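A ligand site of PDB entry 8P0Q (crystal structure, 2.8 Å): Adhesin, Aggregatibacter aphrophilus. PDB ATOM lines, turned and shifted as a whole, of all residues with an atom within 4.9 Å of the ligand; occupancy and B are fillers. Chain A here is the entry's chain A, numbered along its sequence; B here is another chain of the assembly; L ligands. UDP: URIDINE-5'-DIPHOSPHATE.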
ATOM      1  N   SER A 275     -37.239 -18.964   1.467  1.00  0.00           N
ATOM      2  CA  SER A 275     -36.561 -18.643   2.762  1.00  0.00           C
ATOM      3  C   SER A 275     -35.090 -19.099   2.776  1.00  0.00           C
ATOM      4  O   SER A 275     -34.405 -18.792   3.814  1.00  0.00           O
ATOM      5  CB  SER A 275     -37.326 -19.214   3.919  1.00  0.00           C
ATOM      6  OG  SER A 275     -37.340 -20.618   3.790  1.00  0.00           O
ATOM      7  N   SER A 277     -31.040 -19.048   1.593  1.00  0.00           N
ATOM      8  CA  SER A 277     -29.926 -18.155   1.222  1.00  0.00           C
ATOM      9  C   SER A 277     -29.873 -17.910  -0.284  1.00  0.00           C
ATOM     10  O   SER A 277     -29.594 -16.803  -0.690  1.00  0.00           O
ATOM     11  CB  SER A 277     -28.590 -18.695   1.668  1.00  0.00           C
ATOM     12  OG  SER A 277     -28.470 -18.581   3.083  1.00  0.00           O
ATOM     13  N   ARG A 280     -32.707 -15.689  -1.823  1.00  0.00           N
ATOM     14  CA  ARG A 280     -32.521 -14.328  -1.284  1.00  0.00           C
ATOM     15  C   ARG A 280     -31.518 -13.576  -2.181  1.00  0.00           C
ATOM     16  O   ARG A 280     -31.878 -12.497  -2.674  1.00  0.00           O
ATOM     17  CB  ARG A 280     -32.154 -14.432   0.211  1.00  0.00           C
ATOM     18  CG  ARG A 280     -33.331 -14.920   1.073  1.00  0.00           C
ATOM     19  CD  ARG A 280     -32.983 -15.364   2.489  1.00  0.00           C
ATOM     20  NE  ARG A 280     -32.159 -14.348   3.123  1.00  0.00           N
ATOM     21  CZ  ARG A 280     -31.704 -14.360   4.374  1.00  0.00           C
ATOM     22  NH1 ARG A 280     -31.925 -15.386   5.186  1.00  0.00           N
ATOM     23  NH2 ARG A 280     -30.977 -13.346   4.810  1.00  0.00           N
ATOM     24  N   THR A 437     -22.294 -20.479  10.807  1.00  0.00           N
ATOM     25  CA  THR A 437     -22.562 -21.928  10.726  1.00  0.00           C
ATOM     26  C   THR A 437     -21.371 -22.643  11.364  1.00  0.00           C
ATOM     27  O   THR A 437     -20.291 -22.047  11.391  1.00  0.00           O
ATOM     28  CB  THR A 437     -22.776 -22.362   9.271  1.00  0.00           C
ATOM     29  OG1 THR A 437     -22.763 -21.205   8.443  1.00  0.00           O
ATOM     30  CG2 THR A 437     -24.089 -23.093   9.073  1.00  0.00           C
ATOM     31  N   LYS A 440     -17.890 -22.364   9.949  1.00  0.00           N
ATOM     32  CA  LYS A 440     -17.075 -21.133   9.909  1.00  0.00           C
ATOM     33  C   LYS A 440     -16.290 -20.942  11.226  1.00  0.00           C
ATOM     34  O   LYS A 440     -15.460 -19.988  11.309  1.00  0.00           O
ATOM     35  CB  LYS A 440     -17.982 -19.928   9.643  1.00  0.00           C
ATOM     36  CG  LYS A 440     -18.900 -20.096   8.461  1.00  0.00           C
ATOM     37  CD  LYS A 440     -19.563 -18.791   8.116  1.00  0.00           C
ATOM     38  CE  LYS A 440     -20.710 -18.956   7.141  1.00  0.00           C
ATOM     39  NZ  LYS A 440     -21.433 -17.685   6.977  1.00  0.00           N
ATOM     40  N   ALA A 465     -25.193 -17.702  17.542  1.00  0.00           N
ATOM     41  CA  ALA A 465     -26.386 -18.274  16.876  1.00  0.00           C
ATOM     42  C   ALA A 465     -25.877 -19.246  15.813  1.00  0.00           C
ATOM     43  O   ALA A 465     -25.364 -18.764  14.828  1.00  0.00           O
ATOM     44  CB  ALA A 465     -27.225 -17.150  16.328  1.00  0.00           C
ATOM     45  N   LEU A 466     -25.898 -20.550  16.087  1.00  0.00           N
ATOM     46  CA  LEU A 466     -25.069 -21.592  15.389  1.00  0.00           C
ATOM     47  C   LEU A 466     -25.925 -22.431  14.432  1.00  0.00           C
ATOM     48  O   LEU A 466     -26.459 -23.476  14.864  1.00  0.00           O
ATOM     49  CB  LEU A 466     -24.440 -22.506  16.434  1.00  0.00           C
ATOM     50  CG  LEU A 466     -23.403 -21.875  17.354  1.00  0.00           C
ATOM     51  CD1 LEU A 466     -23.053 -22.860  18.453  1.00  0.00           C
ATOM     52  CD2 LEU A 466     -22.146 -21.472  16.584  1.00  0.00           C
ATOM     53  N   GLY A 467     -26.008 -22.019  13.177  1.00  0.00           N
ATOM     54  CA  GLY A 467     -26.551 -22.863  12.109  1.00  0.00           C
ATOM     55  C   GLY A 467     -25.848 -24.218  12.086  1.00  0.00           C
ATOM     56  O   GLY A 467     -24.610 -24.266  12.348  1.00  0.00           O
ATOM     57  N   PRO A 493     -28.282 -23.389  20.104  1.00  0.00           N
ATOM     58  CA  PRO A 493     -28.506 -24.311  18.992  1.00  0.00           C
ATOM     59  C   PRO A 493     -29.209 -23.680  17.782  1.00  0.00           C
ATOM     60  O   PRO A 493     -29.828 -22.647  17.896  1.00  0.00           O
ATOM     61  CB  PRO A 493     -29.406 -25.384  19.604  1.00  0.00           C
ATOM     62  CG  PRO A 493     -29.047 -25.340  21.074  1.00  0.00           C
ATOM     63  CD  PRO A 493     -28.818 -23.866  21.375  1.00  0.00           C
ATOM     64  N   HIS A 494     -29.079 -24.326  16.646  1.00  0.00           N
ATOM     65  CA  HIS A 494     -29.910 -24.041  15.444  1.00  0.00           C
ATOM     66  C   HIS A 494     -31.331 -23.825  15.944  1.00  0.00           C
ATOM     67  O   HIS A 494     -31.782 -24.604  16.752  1.00  0.00           O
ATOM     68  CB  HIS A 494     -29.781 -25.191  14.465  1.00  0.00           C
ATOM     69  CG  HIS A 494     -30.297 -24.872  13.118  1.00  0.00           C
ATOM     70  ND1 HIS A 494     -31.620 -25.029  12.816  1.00  0.00           N
ATOM     71  CD2 HIS A 494     -29.693 -24.405  12.024  1.00  0.00           C
ATOM     72  CE1 HIS A 494     -31.813 -24.679  11.566  1.00  0.00           C
ATOM     73  NE2 HIS A 494     -30.650 -24.281  11.066  1.00  0.00           N
ATOM     74  N   SER A 495     -31.947 -22.721  15.562  1.00  0.00           N
ATOM     75  CA  SER A 495     -33.309 -22.294  15.983  1.00  0.00           C
ATOM     76  C   SER A 495     -34.086 -21.926  14.721  1.00  0.00           C
ATOM     77  O   SER A 495     -33.492 -21.616  13.682  1.00  0.00           O
ATOM     78  CB  SER A 495     -33.214 -21.136  16.970  1.00  0.00           C
ATOM     79  OG  SER A 495     -31.954 -20.489  16.903  1.00  0.00           O
ATOM     80  N   PRO A 496     -35.440 -21.916  14.775  1.00  0.00           N
ATOM     81  CA  PRO A 496     -36.219 -21.351  13.680  1.00  0.00           C
ATOM     82  C   PRO A 496     -35.938 -19.839  13.547  1.00  0.00           C
ATOM     83  O   PRO A 496     -35.634 -19.200  14.534  1.00  0.00           O
ATOM     84  CB  PRO A 496     -37.665 -21.663  14.100  1.00  0.00           C
ATOM     85  CG  PRO A 496     -37.555 -22.730  15.180  1.00  0.00           C
ATOM     86  CD  PRO A 496     -36.269 -22.369  15.906  1.00  0.00           C
ATOM     87  N   TYR A 497     -36.043 -19.303  12.325  1.00  0.00           N
ATOM     88  CA  TYR A 497     -35.601 -17.931  11.935  1.00  0.00           C
ATOM     89  C   TYR A 497     -36.068 -16.867  12.930  1.00  0.00           C
ATOM     90  O   TYR A 497     -35.285 -16.003  13.285  1.00  0.00           O
ATOM     91  CB  TYR A 497     -36.133 -17.527  10.553  1.00  0.00           C
ATOM     92  CG  TYR A 497     -35.487 -16.296   9.953  1.00  0.00           C
ATOM     93  CD1 TYR A 497     -34.179 -16.335   9.501  1.00  0.00           C
ATOM     94  CD2 TYR A 497     -36.185 -15.099   9.826  1.00  0.00           C
ATOM     95  CE1 TYR A 497     -33.569 -15.230   8.933  1.00  0.00           C
ATOM     96  CE2 TYR A 497     -35.596 -13.986   9.250  1.00  0.00           C
ATOM     97  CZ  TYR A 497     -34.283 -14.056   8.803  1.00  0.00           C
ATOM     98  OH  TYR A 497     -33.665 -12.989   8.227  1.00  0.00           O
ATOM     99  N   TYR A 500     -33.923 -17.203  16.004  1.00  0.00           N
ATOM    100  CA  TYR A 500     -32.523 -16.850  15.645  1.00  0.00           C
ATOM    101  C   TYR A 500     -32.353 -15.322  15.654  1.00  0.00           C
ATOM    102  O   TYR A 500     -31.308 -14.851  16.160  1.00  0.00           O
ATOM    103  CB  TYR A 500     -32.134 -17.541  14.343  1.00  0.00           C
ATOM    104  CG  TYR A 500     -31.031 -16.930  13.527  1.00  0.00           C
ATOM    105  CD1 TYR A 500     -29.698 -17.215  13.763  1.00  0.00           C
ATOM    106  CD2 TYR A 500     -31.318 -16.113  12.445  1.00  0.00           C
ATOM    107  CE1 TYR A 500     -28.686 -16.650  12.995  1.00  0.00           C
ATOM    108  CE2 TYR A 500     -30.325 -15.557  11.647  1.00  0.00           C
ATOM    109  CZ  TYR A 500     -29.004 -15.822  11.938  1.00  0.00           C
ATOM    110  OH  TYR A 500     -28.039 -15.283  11.149  1.00  0.00           O
ATOM    111  N   PHE A 516     -13.823 -17.478   6.367  1.00  0.00           N
ATOM    112  CA  PHE A 516     -15.047 -17.486   5.525  1.00  0.00           C
ATOM    113  C   PHE A 516     -16.104 -16.634   6.245  1.00  0.00           C
ATOM    114  O   PHE A 516     -16.530 -17.072   7.303  1.00  0.00           O
ATOM    115  CB  PHE A 516     -15.449 -18.941   5.339  1.00  0.00           C
ATOM    116  CG  PHE A 516     -16.523 -19.178   4.317  1.00  0.00           C
ATOM    117  CD1 PHE A 516     -17.727 -18.504   4.394  1.00  0.00           C
ATOM    118  CD2 PHE A 516     -16.332 -20.126   3.318  1.00  0.00           C
ATOM    119  CE1 PHE A 516     -18.709 -18.727   3.450  1.00  0.00           C
ATOM    120  CE2 PHE A 516     -17.316 -20.340   2.375  1.00  0.00           C
ATOM    121  CZ  PHE A 516     -18.504 -19.642   2.446  1.00  0.00           C
ATOM    122  N   GLY A 517     -16.518 -15.492   5.684  1.00  0.00           N
ATOM    123  CA  GLY A 517     -17.459 -14.565   6.338  1.00  0.00           C
ATOM    124  C   GLY A 517     -18.926 -14.823   5.997  1.00  0.00           C
ATOM    125  O   GLY A 517     -19.245 -15.823   5.325  1.00  0.00           O
ATOM    126  N   ASN A 518     -19.767 -13.865   6.407  1.00  0.00           N
ATOM    127  CA  ASN A 518     -21.249 -13.855   6.275  1.00  0.00           C
ATOM    128  C   ASN A 518     -21.694 -13.086   5.022  1.00  0.00           C
ATOM    129  O   ASN A 518     -20.872 -12.357   4.406  1.00  0.00           O
ATOM    130  CB  ASN A 518     -21.934 -13.177   7.471  1.00  0.00           C
ATOM    131  CG  ASN A 518     -21.688 -13.844   8.815  1.00  0.00           C
ATOM    132  OD1 ASN A 518     -21.256 -14.995   8.874  1.00  0.00           O
ATOM    133  ND2 ASN A 518     -21.987 -13.125   9.892  1.00  0.00           N
ATOM    134  N   THR A 519     -22.980 -13.230   4.689  1.00  0.00           N
ATOM    135  CA  THR A 519     -23.703 -12.587   3.563  1.00  0.00           C
ATOM    136  C   THR A 519     -25.139 -12.351   4.047  1.00  0.00           C
ATOM    137  O   THR A 519     -25.418 -11.280   4.574  1.00  0.00           O
ATOM    138  CB  THR A 519     -23.643 -13.472   2.309  1.00  0.00           C
ATOM    139  OG1 THR A 519     -22.309 -13.974   2.212  1.00  0.00           O
ATOM    140  CG2 THR A 519     -24.031 -12.741   1.035  1.00  0.00           C
ATOM    141  N   ASN A 520     -25.984 -13.384   3.991  1.00  0.00           N
ATOM    142  CA  ASN A 520     -27.334 -13.421   4.585  1.00  0.00           C
ATOM    143  C   ASN A 520     -27.212 -13.039   6.057  1.00  0.00           C
ATOM    144  O   ASN A 520     -28.118 -12.375   6.542  1.00  0.00           O
ATOM    145  CB  ASN A 520     -28.011 -14.777   4.372  1.00  0.00           C
ATOM    146  CG  ASN A 520     -28.160 -15.124   2.908  1.00  0.00           C
ATOM    147  OD1 ASN A 520     -29.179 -14.836   2.288  1.00  0.00           O
ATOM    148  ND2 ASN A 520     -27.130 -15.707   2.328  1.00  0.00           N
ATOM    149  N   GLY A 521     -26.124 -13.419   6.738  1.00  0.00           N
ATOM    150  CA  GLY A 521     -25.868 -13.051   8.139  1.00  0.00           C
ATOM    151  C   GLY A 521     -25.750 -11.545   8.330  1.00  0.00           C
ATOM    152  O   GLY A 521     -25.991 -11.071   9.443  1.00  0.00           O
ATOM    153  N   ASP A 524     -29.234 -10.061   8.076  1.00  0.00           N
ATOM    154  CA  ASP A 524     -29.829 -10.323   9.409  1.00  0.00           C
ATOM    155  C   ASP A 524     -29.378  -9.227  10.364  1.00  0.00           C
ATOM    156  O   ASP A 524     -30.227  -8.719  11.083  1.00  0.00           O
ATOM    157  CB  ASP A 524     -29.499 -11.728   9.909  1.00  0.00           C
ATOM    158  CG  ASP A 524     -29.967 -12.839   8.963  1.00  0.00           C
ATOM    159  OD1 ASP A 524     -30.993 -12.631   8.269  1.00  0.00           O
ATOM    160  OD2 ASP A 524     -29.299 -13.907   8.921  1.00  0.00           O
ATOM    161  N   PHE B   1     -33.272 -22.252   6.401  1.00  0.00           N
ATOM    162  CA  PHE B   1     -32.345 -23.029   5.540  1.00  0.00           C
ATOM    163  C   PHE B   1     -31.262 -22.056   4.981  1.00  0.00           C
ATOM    164  O   PHE B   1     -31.606 -21.093   4.284  1.00  0.00           O
ATOM    165  CB  PHE B   1     -33.179 -23.786   4.494  1.00  0.00           C
ATOM    166  CG  PHE B   1     -32.824 -25.230   4.163  1.00  0.00           C
ATOM    167  CD1 PHE B   1     -31.497 -25.651   4.009  1.00  0.00           C
ATOM    168  CD2 PHE B   1     -33.826 -26.163   3.910  1.00  0.00           C
ATOM    169  CE1 PHE B   1     -31.189 -26.958   3.673  1.00  0.00           C
ATOM    170  CE2 PHE B   1     -33.516 -27.479   3.563  1.00  0.00           C
ATOM    171  CZ  PHE B   1     -32.202 -27.879   3.454  1.00  0.00           C
ATOM    172  N   GLY B   2     -29.984 -22.305   5.308  1.00  0.00           N
ATOM    173  CA  GLY B   2     -28.779 -21.659   4.736  1.00  0.00           C
ATOM    174  C   GLY B   2     -27.850 -22.639   4.022  1.00  0.00           C
ATOM    175  O   GLY B   2     -28.260 -23.799   3.745  1.00  0.00           O
ATOM    176  N   ASN B   3     -26.624 -22.171   3.713  1.00  0.00           N
ATOM    177  CA  ASN B   3     -25.599 -22.825   2.847  1.00  0.00           C
ATOM    178  C   ASN B   3     -24.897 -23.946   3.627  1.00  0.00           C
ATOM    179  O   ASN B   3     -24.049 -23.615   4.476  1.00  0.00           O
ATOM    180  CB  ASN B   3     -24.480 -21.862   2.376  1.00  0.00           C
ATOM    181  CG  ASN B   3     -24.874 -20.914   1.262  1.00  0.00           C
ATOM    182  OD1 ASN B   3     -25.716 -21.268   0.439  1.00  0.00           O
ATOM    183  ND2 ASN B   3     -24.297 -19.717   1.230  1.00  0.00           N
HETATM  184  N1  UDP L   1     -30.313 -19.624  10.121  1.00  0.00           N
HETATM  185  C2  UDP L   1     -31.471 -19.855  10.843  1.00  0.00           C
HETATM  186  N3  UDP L   1     -31.293 -20.278  12.142  1.00  0.00           N
HETATM  187  C4  UDP L   1     -30.090 -20.464  12.779  1.00  0.00           C
HETATM  188  C5  UDP L   1     -28.940 -20.149  11.990  1.00  0.00           C
HETATM  189  C6  UDP L   1     -29.089 -19.766  10.713  1.00  0.00           C
HETATM  190  O2  UDP L   1     -32.582 -19.710  10.346  1.00  0.00           O
HETATM  191  O4  UDP L   1     -30.072 -20.811  13.958  1.00  0.00           O
HETATM  192  C1' UDP L   1     -30.502 -19.213   8.709  1.00  0.00           C
HETATM  193  C2' UDP L   1     -30.903 -17.751   8.620  1.00  0.00           C
HETATM  194  O2' UDP L   1     -31.937 -17.697   7.686  1.00  0.00           O
HETATM  195  C3' UDP L   1     -29.615 -17.096   8.136  1.00  0.00           C
HETATM  196  C4' UDP L   1     -29.101 -18.180   7.186  1.00  0.00           C
HETATM  197  O4' UDP L   1     -29.321 -19.383   7.947  1.00  0.00           O
HETATM  198  O3' UDP L   1     -29.797 -15.862   7.425  1.00  0.00           O
HETATM  199  C5' UDP L   1     -27.677 -17.971   6.739  1.00  0.00           C
HETATM  200  O5' UDP L   1     -26.892 -19.154   6.822  1.00  0.00           O
HETATM  201  PA  UDP L   1     -25.686 -19.225   5.771  1.00  0.00           P
HETATM  202  O1A UDP L   1     -24.823 -20.398   6.156  1.00  0.00           O
HETATM  203  O2A UDP L   1     -26.212 -19.181   4.387  1.00  0.00           O
HETATM  204  O3A UDP L   1     -24.902 -17.848   5.971  1.00  0.00           O
HETATM  205  PB  UDP L   1     -24.384 -16.700   4.968  1.00  0.00           P
HETATM  206  O1B UDP L   1     -24.431 -15.415   5.742  1.00  0.00           O
HETATM  207  O2B UDP L   1     -25.026 -16.893   3.632  1.00  0.00           O
HETATM  208  O3B UDP L   1     -22.818 -16.993   4.751  1.00  0.00           O
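The side-chain hydroxyl of Ser 277 is in hydrogen-bond range of the side-chain amide nitrogen of Asn 520, at 3.3 Å.
The side-chain amino group of Lys 440 is in hydrogen-bond range of the side-chain amide oxygen of Asn 518 (3.3 Å).
The side-chain carboxylate (OD2) of Asp 524 sits at hydrogen-bond distance from the side-chain hydroxyl (OH) of Tyr 500, at 2.9 Å.
The backbone NH (N) of His 494 sits at hydrogen-bond distance from the backbone carbonyl oxygen (O) of Leu 466.
The guanidinium group (NE) of Arg 280 sits at hydrogen-bond distance from the side-chain amide oxygen (OD1) of Asn 520 (3.1 Å).
The side-chain hydroxyl (OH) of Tyr 497 lies within hydrogen-bond range of the side-chain carboxylate (OD1) of Asp 524, at 2.7 Å.
The backbone NH of Ser 277 is in hydrogen-bond range of the backbone carbonyl oxygen of Phe 1 of chain B (3.4 Å).
NZ of Lys 440 sits at hydrogen-bond distance from O of Gly 517 (3.3 Å).
The side-chain amide nitrogen (ND2) of Asn 520 sits at hydrogen-bond distance from an oxygen (O2B) of the ligand (2.7 Å).
OG of Ser 277 lies within hydrogen-bond range of O2A of the ligand (2.7 Å).
O1B of the ligand is in hydrogen-bond range of N of Thr 519.
The side-chain amino group (NZ) of Lys 440 is in salt-bridge range of an oxygen (O3B) of the ligand.
OD2 of Asp 524 is in hydrogen-bond range of O3' of the ligand, at 2.5 Å.
N of Gly 521 is in hydrogen-bond range of O1B of the ligand, 2.8 Å away.
The backbone NH (N) of Asn 520 is in hydrogen-bond range of an oxygen (O1B) of the ligand (3.1 Å).
An oxygen (O2A) of the ligand lies within hydrogen-bond range of the backbone NH (N) of Asn 3 of chain B (3.1 Å).
The side-chain hydroxyl (OG1) of Thr 437 sits at hydrogen-bond distance from an oxygen (O1A) of the ligand.
An oxygen (O3') of the ligand sits at hydrogen-bond distance from the guanidinium group (NH1) of Arg 280.
A nitrogen (N3) of the ligand is in hydrogen-bond range of the backbone carbonyl oxygen (O) of Ser 495, 3.0 Å away.
N of Ser 495 sits at hydrogen-bond distance from O4 of the ligand (3.1 Å).
Gly 467 touches the ligand (CA to C5, 3.6 Å).
His 494 touches the ligand (CA to O4, 3.6 Å).
CD1 of Tyr 497 touches O2' of the ligand (3.2 Å).
Tyr 500 touches the ligand (CD1 to C4, 3.4 Å).
Gly 517 touches the ligand (O to O3B, 3.8 Å).
Asn 518 touches the ligand (CA to O1B, 3.6 Å).
Gly 2 of chain B touches the ligand (CA to O2A, 3.6 Å).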
